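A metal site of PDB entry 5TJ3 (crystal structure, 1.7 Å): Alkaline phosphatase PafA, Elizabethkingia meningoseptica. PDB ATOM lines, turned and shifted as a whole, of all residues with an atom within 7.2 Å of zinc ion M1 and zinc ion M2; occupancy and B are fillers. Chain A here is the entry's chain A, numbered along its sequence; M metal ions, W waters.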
ATOM      1  N   VAL A  25     -11.758 -36.133  14.685  1.00  0.00           N
ATOM      2  CA  VAL A  25     -12.615 -35.007  15.008  1.00  0.00           C
ATOM      3  C   VAL A  25     -13.742 -34.970  13.981  1.00  0.00           C
ATOM      4  O   VAL A  25     -13.505 -34.816  12.777  1.00  0.00           O
ATOM      5  CB  VAL A  25     -11.839 -33.682  15.084  1.00  0.00           C
ATOM      6  CG1 VAL A  25     -10.423 -33.825  14.562  1.00  0.00           C
ATOM      7  CG2 VAL A  25     -12.601 -32.515  14.463  1.00  0.00           C
ATOM      8  N   VAL A  26     -14.969 -35.181  14.466  1.00  0.00           N
ATOM      9  CA  VAL A  26     -16.156 -35.224  13.624  1.00  0.00           C
ATOM     10  C   VAL A  26     -16.631 -33.787  13.450  1.00  0.00           C
ATOM     11  O   VAL A  26     -17.051 -33.132  14.410  1.00  0.00           O
ATOM     12  CB  VAL A  26     -17.258 -36.086  14.246  1.00  0.00           C
ATOM     13  CG1 VAL A  26     -18.474 -36.131  13.332  1.00  0.00           C
ATOM     14  CG2 VAL A  26     -16.723 -37.485  14.513  1.00  0.00           C
ATOM     15  N   ASP A  27     -16.551 -33.291  12.224  1.00  0.00           N
ATOM     16  CA  ASP A  27     -16.775 -31.880  11.964  1.00  0.00           C
ATOM     17  C   ASP A  27     -18.231 -31.515  12.230  1.00  0.00           C
ATOM     18  O   ASP A  27     -19.152 -32.146  11.706  1.00  0.00           O
ATOM     19  CB  ASP A  27     -16.382 -31.564  10.524  1.00  0.00           C
ATOM     20  CG  ASP A  27     -15.984 -30.130  10.341  1.00  0.00           C
ATOM     21  OD1 ASP A  27     -16.692 -29.266  10.891  1.00  0.00           O
ATOM     22  OD2 ASP A  27     -14.970 -29.874   9.662  1.00  0.00           O
ATOM     23  N   GLN A  28     -18.434 -30.501  13.078  1.00  0.00           N
ATOM     24  CA  GLN A  28     -19.740 -29.954  13.440  1.00  0.00           C
ATOM     25  C   GLN A  28     -20.562 -30.899  14.313  1.00  0.00           C
ATOM     26  O   GLN A  28     -21.789 -30.781  14.368  1.00  0.00           O
ATOM     27  CB  GLN A  28     -20.559 -29.558  12.195  1.00  0.00           C
ATOM     28  CG  GLN A  28     -21.544 -28.427  12.443  1.00  0.00           C
ATOM     29  CD  GLN A  28     -22.496 -28.218  11.273  1.00  0.00           C
ATOM     30  OE1 GLN A  28     -23.666 -28.604  11.352  1.00  0.00           O
ATOM     31  NE2 GLN A  28     -22.003 -27.614  10.200  1.00  0.00           N
ATOM     32  N   MET A  29     -19.927 -31.842  15.005  1.00  0.00           N
ATOM     33  CA  MET A  29     -20.688 -32.789  15.825  1.00  0.00           C
ATOM     34  C   MET A  29     -21.027 -32.149  17.160  1.00  0.00           C
ATOM     35  O   MET A  29     -20.176 -32.018  18.034  1.00  0.00           O
ATOM     36  CB  MET A  29     -19.904 -34.080  16.023  1.00  0.00           C
ATOM     37  CG  MET A  29     -20.688 -35.082  16.831  1.00  0.00           C
ATOM     38  SD  MET A  29     -19.872 -36.681  16.944  1.00  0.00           S
ATOM     39  CE  MET A  29     -21.104 -37.587  17.876  1.00  0.00           C
ATOM     40  N   THR A  66     -16.039 -20.204  16.967  1.00  0.00           N
ATOM     41  CA  THR A  66     -16.023 -21.666  16.938  1.00  0.00           C
ATOM     42  C   THR A  66     -16.144 -22.162  15.491  1.00  0.00           C
ATOM     43  O   THR A  66     -17.160 -22.682  15.056  1.00  0.00           O
ATOM     44  CB  THR A  66     -17.112 -22.236  17.831  1.00  0.00           C
ATOM     45  OG1 THR A  66     -18.367 -21.592  17.526  1.00  0.00           O
ATOM     46  CG2 THR A  66     -16.779 -22.003  19.294  1.00  0.00           C
ATOM     47  N   VAL A  67     -15.043 -21.976  14.751  1.00  0.00           N
ATOM     48  CA  VAL A  67     -14.961 -22.431  13.374  1.00  0.00           C
ATOM     49  C   VAL A  67     -13.918 -23.542  13.226  1.00  0.00           C
ATOM     50  O   VAL A  67     -13.239 -23.887  14.189  1.00  0.00           O
ATOM     51  CB  VAL A  67     -14.654 -21.262  12.426  1.00  0.00           C
ATOM     52  CG1 VAL A  67     -15.710 -20.182  12.574  1.00  0.00           C
ATOM     53  CG2 VAL A  67     -13.271 -20.710  12.691  1.00  0.00           C
ATOM     54  N   TPO A  68     -13.795 -24.081  12.015  1.00  0.00           N
ATOM     55  CA  TPO A  68     -13.006 -25.288  11.751  1.00  0.00           C
ATOM     56  CB  TPO A  68     -13.268 -25.791  10.348  1.00  0.00           C
ATOM     57  CG2 TPO A  68     -12.255 -26.860   9.942  1.00  0.00           C
ATOM     58  OG1 TPO A  68     -14.557 -26.363  10.322  1.00  0.00           O
ATOM     59  P   TPO A  68     -15.438 -25.454   9.324  1.00  0.00           P
ATOM     60  O1P TPO A  68     -15.426 -24.029   9.746  1.00  0.00           O
ATOM     61  O2P TPO A  68     -14.822 -25.580   7.846  1.00  0.00           O
ATOM     62  O3P TPO A  68     -16.930 -26.032   9.363  1.00  0.00           O
ATOM     63  C   TPO A  68     -11.508 -25.149  11.978  1.00  0.00           C
ATOM     64  O   TPO A  68     -10.914 -25.930  12.731  1.00  0.00           O
ATOM     65  N   ALA A  69     -10.899 -24.185  11.300  1.00  0.00           N
ATOM     66  CA  ALA A  69      -9.446 -24.023  11.340  1.00  0.00           C
ATOM     67  C   ALA A  69      -8.969 -23.895  12.776  1.00  0.00           C
ATOM     68  O   ALA A  69      -7.975 -24.515  13.156  1.00  0.00           O
ATOM     69  CB  ALA A  69      -9.010 -22.830  10.520  1.00  0.00           C
ATOM     70  N   GLY A  71     -10.674 -24.830  15.536  1.00  0.00           N
ATOM     71  CA  GLY A  71     -11.009 -26.033  16.285  1.00  0.00           C
ATOM     72  C   GLY A  71      -9.964 -27.122  16.140  1.00  0.00           C
ATOM     73  O   GLY A  71      -9.490 -27.675  17.132  1.00  0.00           O
ATOM     74  N   HIS A  72      -9.585 -27.425  14.901  1.00  0.00           N
ATOM     75  CA  HIS A  72      -8.554 -28.441  14.688  1.00  0.00           C
ATOM     76  C   HIS A  72      -7.213 -27.979  15.238  1.00  0.00           C
ATOM     77  O   HIS A  72      -6.466 -28.778  15.818  1.00  0.00           O
ATOM     78  CB  HIS A  72      -8.463 -28.783  13.209  1.00  0.00           C
ATOM     79  CG  HIS A  72      -9.617 -29.592  12.704  1.00  0.00           C
ATOM     80  ND1 HIS A  72     -10.837 -29.040  12.388  1.00  0.00           N
ATOM     81  CD2 HIS A  72      -9.749 -30.926  12.525  1.00  0.00           C
ATOM     82  CE1 HIS A  72     -11.662 -29.991  12.005  1.00  0.00           C
ATOM     83  NE2 HIS A  72     -11.027 -31.147  12.073  1.00  0.00           N
ATOM     84  N   ASN A  89     -10.941 -19.585   9.876  1.00  0.00           N
ATOM     85  CA  ASN A  89     -10.736 -20.130   8.541  1.00  0.00           C
ATOM     86  C   ASN A  89     -10.117 -19.080   7.622  1.00  0.00           C
ATOM     87  O   ASN A  89      -9.286 -19.387   6.776  1.00  0.00           O
ATOM     88  CB  ASN A  89     -12.048 -20.629   7.950  1.00  0.00           C
ATOM     89  CG  ASN A  89     -12.632 -21.793   8.729  1.00  0.00           C
ATOM     90  OD1 ASN A  89     -11.913 -22.548   9.367  1.00  0.00           O
ATOM     91  ND2 ASN A  89     -13.954 -21.948   8.676  1.00  0.00           N
ATOM     92  N   LYS A 151     -11.035 -31.643   3.735  1.00  0.00           N
ATOM     93  CA  LYS A 151     -10.674 -30.234   3.782  1.00  0.00           C
ATOM     94  C   LYS A 151      -9.176 -30.083   4.016  1.00  0.00           C
ATOM     95  O   LYS A 151      -8.606 -30.747   4.888  1.00  0.00           O
ATOM     96  CB  LYS A 151     -11.422 -29.493   4.892  1.00  0.00           C
ATOM     97  CG  LYS A 151     -12.925 -29.637   4.899  1.00  0.00           C
ATOM     98  CD  LYS A 151     -13.488 -28.933   6.127  1.00  0.00           C
ATOM     99  CE  LYS A 151     -15.002 -28.936   6.139  1.00  0.00           C
ATOM    100  NZ  LYS A 151     -15.557 -28.147   7.275  1.00  0.00           N
ATOM    101  N   ARG A 153      -7.608 -27.526   5.414  1.00  0.00           N
ATOM    102  CA  ARG A 153      -7.331 -26.983   6.750  1.00  0.00           C
ATOM    103  C   ARG A 153      -7.435 -28.062   7.817  1.00  0.00           C
ATOM    104  O   ARG A 153      -6.665 -28.061   8.789  1.00  0.00           O
ATOM    105  CB  ARG A 153      -8.276 -25.826   7.053  1.00  0.00           C
ATOM    106  CG  ARG A 153      -9.765 -26.130   6.871  1.00  0.00           C
ATOM    107  CD  ARG A 153     -10.600 -24.871   7.064  1.00  0.00           C
ATOM    108  NE  ARG A 153     -12.033 -25.089   6.896  1.00  0.00           N
ATOM    109  CZ  ARG A 153     -12.662 -24.987   5.730  1.00  0.00           C
ATOM    110  NH1 ARG A 153     -11.997 -24.679   4.632  1.00  0.00           N
ATOM    111  NH2 ARG A 153     -13.978 -25.199   5.665  1.00  0.00           N
ATOM    112  N   ALA A 154      -8.374 -28.988   7.668  1.00  0.00           N
ATOM    113  CA  ALA A 154      -8.613 -30.011   8.683  1.00  0.00           C
ATOM    114  C   ALA A 154      -7.634 -31.185   8.588  1.00  0.00           C
ATOM    115  O   ALA A 154      -7.639 -32.043   9.483  1.00  0.00           O
ATOM    116  CB  ALA A 154     -10.047 -30.524   8.584  1.00  0.00           C
ATOM    117  N   ASN A 289     -10.094 -36.003  10.054  1.00  0.00           N
ATOM    118  CA  ASN A 289     -11.288 -35.189  10.231  1.00  0.00           C
ATOM    119  C   ASN A 289     -12.387 -35.748   9.354  1.00  0.00           C
ATOM    120  O   ASN A 289     -12.167 -36.011   8.166  1.00  0.00           O
ATOM    121  CB  ASN A 289     -10.995 -33.734   9.871  1.00  0.00           C
ATOM    122  CG  ASN A 289     -12.229 -32.998   9.376  1.00  0.00           C
ATOM    123  OD1 ASN A 289     -12.523 -32.993   8.181  1.00  0.00           O
ATOM    124  ND2 ASN A 289     -12.941 -32.369  10.292  1.00  0.00           N
ATOM    125  N   ALA A 291     -15.386 -34.669   7.601  1.00  0.00           N
ATOM    126  CA  ALA A 291     -15.894 -33.364   7.219  1.00  0.00           C
ATOM    127  C   ALA A 291     -17.348 -33.374   6.757  1.00  0.00           C
ATOM    128  O   ALA A 291     -18.002 -32.318   6.798  1.00  0.00           O
ATOM    129  CB  ALA A 291     -15.028 -32.753   6.122  1.00  0.00           C
ATOM    130  N   ASP A 294     -20.217 -31.857   8.606  1.00  0.00           N
ATOM    131  CA  ASP A 294     -20.282 -30.396   8.561  1.00  0.00           C
ATOM    132  C   ASP A 294     -20.954 -29.901   7.293  1.00  0.00           C
ATOM    133  O   ASP A 294     -21.788 -29.001   7.334  1.00  0.00           O
ATOM    134  CB  ASP A 294     -18.874 -29.814   8.669  1.00  0.00           C
ATOM    135  CG  ASP A 294     -18.856 -28.311   8.641  1.00  0.00           C
ATOM    136  OD1 ASP A 294     -19.249 -27.692   9.656  1.00  0.00           O
ATOM    137  OD2 ASP A 294     -18.445 -27.742   7.602  1.00  0.00           O
ATOM    138  N   TYR A 295     -20.585 -30.478   6.148  1.00  0.00           N
ATOM    139  CA  TYR A 295     -21.213 -30.091   4.885  1.00  0.00           C
ATOM    140  C   TYR A 295     -22.699 -30.419   4.913  1.00  0.00           C
ATOM    141  O   TYR A 295     -23.539 -29.581   4.552  1.00  0.00           O
ATOM    142  CB  TYR A 295     -20.521 -30.784   3.716  1.00  0.00           C
ATOM    143  CG  TYR A 295     -19.173 -30.195   3.399  1.00  0.00           C
ATOM    144  CD1 TYR A 295     -19.060 -28.997   2.715  1.00  0.00           C
ATOM    145  CD2 TYR A 295     -18.000 -30.839   3.778  1.00  0.00           C
ATOM    146  CE1 TYR A 295     -17.825 -28.445   2.421  1.00  0.00           C
ATOM    147  CE2 TYR A 295     -16.756 -30.307   3.490  1.00  0.00           C
ATOM    148  CZ  TYR A 295     -16.683 -29.106   2.805  1.00  0.00           C
ATOM    149  OH  TYR A 295     -15.458 -28.554   2.511  1.00  0.00           O
ATOM    150  N   HIS A 298     -24.416 -28.066   7.406  1.00  0.00           N
ATOM    151  CA  HIS A 298     -24.527 -26.712   6.880  1.00  0.00           C
ATOM    152  C   HIS A 298     -25.710 -26.569   5.932  1.00  0.00           C
ATOM    153  O   HIS A 298     -26.362 -25.522   5.881  1.00  0.00           O
ATOM    154  CB  HIS A 298     -23.243 -26.319   6.164  1.00  0.00           C
ATOM    155  CG  HIS A 298     -22.227 -25.656   7.047  1.00  0.00           C
ATOM    156  ND1 HIS A 298     -22.429 -24.407   7.593  1.00  0.00           N
ATOM    157  CD2 HIS A 298     -21.010 -26.068   7.463  1.00  0.00           C
ATOM    158  CE1 HIS A 298     -21.372 -24.087   8.318  1.00  0.00           C
ATOM    159  NE2 HIS A 298     -20.502 -25.072   8.253  1.00  0.00           N
ATOM    160  N   ALA A 340     -14.933 -32.957  18.440  1.00  0.00           N
ATOM    161  CA  ALA A 340     -15.438 -32.149  17.350  1.00  0.00           C
ATOM    162  C   ALA A 340     -14.770 -30.788  17.414  1.00  0.00           C
ATOM    163  O   ALA A 340     -14.304 -30.355  18.470  1.00  0.00           O
ATOM    164  CB  ALA A 340     -16.963 -31.993  17.423  1.00  0.00           C
ATOM    165  N   ASP A 341     -14.702 -30.125  16.268  1.00  0.00           N
ATOM    166  CA  ASP A 341     -14.133 -28.778  16.240  1.00  0.00           C
ATOM    167  C   ASP A 341     -15.136 -27.718  16.650  1.00  0.00           C
ATOM    168  O   ASP A 341     -14.727 -26.577  16.915  1.00  0.00           O
ATOM    169  CB  ASP A 341     -13.571 -28.478  14.849  1.00  0.00           C
ATOM    170  CG  ASP A 341     -14.575 -28.722  13.738  1.00  0.00           C
ATOM    171  OD1 ASP A 341     -15.596 -29.395  13.968  1.00  0.00           O
ATOM    172  OD2 ASP A 341     -14.319 -28.245  12.613  1.00  0.00           O
ATOM    173  N   HIS A 342     -16.424 -28.074  16.729  1.00  0.00           N
ATOM    174  CA  HIS A 342     -17.509 -27.196  17.148  1.00  0.00           C
ATOM    175  C   HIS A 342     -18.836 -27.932  17.008  1.00  0.00           C
ATOM    176  O   HIS A 342     -18.893 -29.016  16.427  1.00  0.00           O
ATOM    177  CB  HIS A 342     -17.548 -25.929  16.292  1.00  0.00           C
ATOM    178  CG  HIS A 342     -17.534 -26.209  14.824  1.00  0.00           C
ATOM    179  ND1 HIS A 342     -18.643 -26.696  14.155  1.00  0.00           N
ATOM    180  CD2 HIS A 342     -16.546 -26.130  13.899  1.00  0.00           C
ATOM    181  CE1 HIS A 342     -18.336 -26.877  12.886  1.00  0.00           C
ATOM    182  NE2 HIS A 342     -17.067 -26.542  12.708  1.00  0.00           N
ATOM    183  N   GLY A 343     -19.904 -27.361  17.553  1.00  0.00           N
ATOM    184  CA  GLY A 343     -21.253 -27.845  17.338  1.00  0.00           C
ATOM    185  C   GLY A 343     -21.932 -27.102  16.207  1.00  0.00           C
ATOM    186  O   GLY A 343     -21.294 -26.726  15.212  1.00  0.00           O
ATOM    187  N   THR A 473     -27.635 -24.339   8.425  1.00  0.00           N
ATOM    188  CA  THR A 473     -27.194 -23.747   9.692  1.00  0.00           C
ATOM    189  C   THR A 473     -25.714 -23.384   9.579  1.00  0.00           C
ATOM    190  O   THR A 473     -25.074 -23.601   8.554  1.00  0.00           O
ATOM    191  CB  THR A 473     -27.461 -24.691  10.871  1.00  0.00           C
ATOM    192  OG1 THR A 473     -27.331 -23.966  12.092  1.00  0.00           O
ATOM    193  CG2 THR A 473     -26.463 -25.850  10.854  1.00  0.00           C
ATOM    194  N   THR A 474     -25.190 -22.818  10.664  1.00  0.00           N
ATOM    195  CA  THR A 474     -23.784 -22.431  10.732  1.00  0.00           C
ATOM    196  C   THR A 474     -23.364 -22.416  12.196  1.00  0.00           C
ATOM    197  O   THR A 474     -24.130 -22.798  13.088  1.00  0.00           O
ATOM    198  CB  THR A 474     -23.551 -21.085  10.040  1.00  0.00           C
ATOM    199  OG1 THR A 474     -22.149 -20.831   9.932  1.00  0.00           O
ATOM    200  CG2 THR A 474     -24.207 -19.962  10.829  1.00  0.00           C
ATOM    201  N   HIS A 475     -22.146 -21.942  12.446  1.00  0.00           N
ATOM    202  CA  HIS A 475     -21.513 -22.082  13.752  1.00  0.00           C
ATOM    203  C   HIS A 475     -20.377 -21.068  13.860  1.00  0.00           C
ATOM    204  O   HIS A 475     -19.604 -20.919  12.911  1.00  0.00           O
ATOM    205  CB  HIS A 475     -20.956 -23.502  13.899  1.00  0.00           C
ATOM    206  CG  HIS A 475     -19.993 -23.857  12.815  1.00  0.00           C
ATOM    207  ND1 HIS A 475     -18.674 -23.452  12.825  1.00  0.00           N
ATOM    208  CD2 HIS A 475     -20.171 -24.529  11.650  1.00  0.00           C
ATOM    209  CE1 HIS A 475     -18.067 -23.888  11.738  1.00  0.00           C
ATOM    210  NE2 HIS A 475     -18.955 -24.539  11.009  1.00  0.00           N
HETATM  211 ZN    ZN M   1     -15.792 -27.588  11.374  1.00  0.00          ZN
HETATM  212 ZN    ZN M   2     -18.741 -25.596   9.140  1.00  0.00          ZN
HETATM  213  O   HOH W   1     -17.649 -23.892   7.786  1.00  0.00           O
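OD1 of Asp 341 sits at hydrogen-bond distance from N of Gln 28.
The backbone carbonyl oxygen (O) of His 342 lies within hydrogen-bond range of the backbone NH (N) of Met 29.
The side-chain amide nitrogen (ND2) of Asn 289 is in hydrogen-bond range of the side-chain carboxylate (OD2) of Asp 27 (3.3 Å).
OD2 of Asp 294 lies within salt-bridge range of NZ of Lys 151, 2.9 Å away.
O2P of TPO 68 is in salt-bridge range of the side-chain amino group (NZ) of Lys 151, 2.7 Å away.
A ring nitrogen (ND1) of His 298 sits at hydrogen-bond distance from the backbone carbonyl oxygen of Thr 473 (2.9 Å).
The side-chain amide nitrogen (NE2) of Gln 28 is in hydrogen-bond range of the backbone carbonyl oxygen (O) of Asp 294, at 3.2 Å.
O of Asp 27 lies within hydrogen-bond range of N of Asp 294, 3.3 Å away.
Five residues have an atom within 4 Å of zinc ion M1: Asp 27, TPO 68, Asp 294, Asp 341 and His 342.
Gln 28 touches zinc ion M2.
Six residues have an atom within 4 Å of zinc ion M2: Gln 28, TPO 68, Asp 294, His 298, His 342 and His 475.
Along chain A the residues within 4 Å of zinc ion M2 span positions 28 to 475.
The nearest printed residue that does not touch zinc ion M2 is Lys 151 (4.5 Å).
Zinc ion M1 is bound by OD1 of Asp 27 (2.0 Å), OG1 of TPO 68 (2.0 Å), OD2 of Asp 341 (2.0 Å) and NE2 of His 342 (2.1 Å).
Zinc ion M1 has four donor atoms within binding distance.
Slightly farther from zinc ion M1 lies O3P of TPO 68 (2.8 Å).
Zinc ion M2 is bound by O3P of TPO 68 (1.9 Å), NE2 of His 298 (2.0 Å), NE2 of His 475 (2.2 Å), OD1 of Asp 294 (2.2 Å) and water W1 (2.4 Å).
Slightly farther from zinc ion M2 lies the side-chain carboxylate (OD2) of Asp 294 (2.7 Å).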
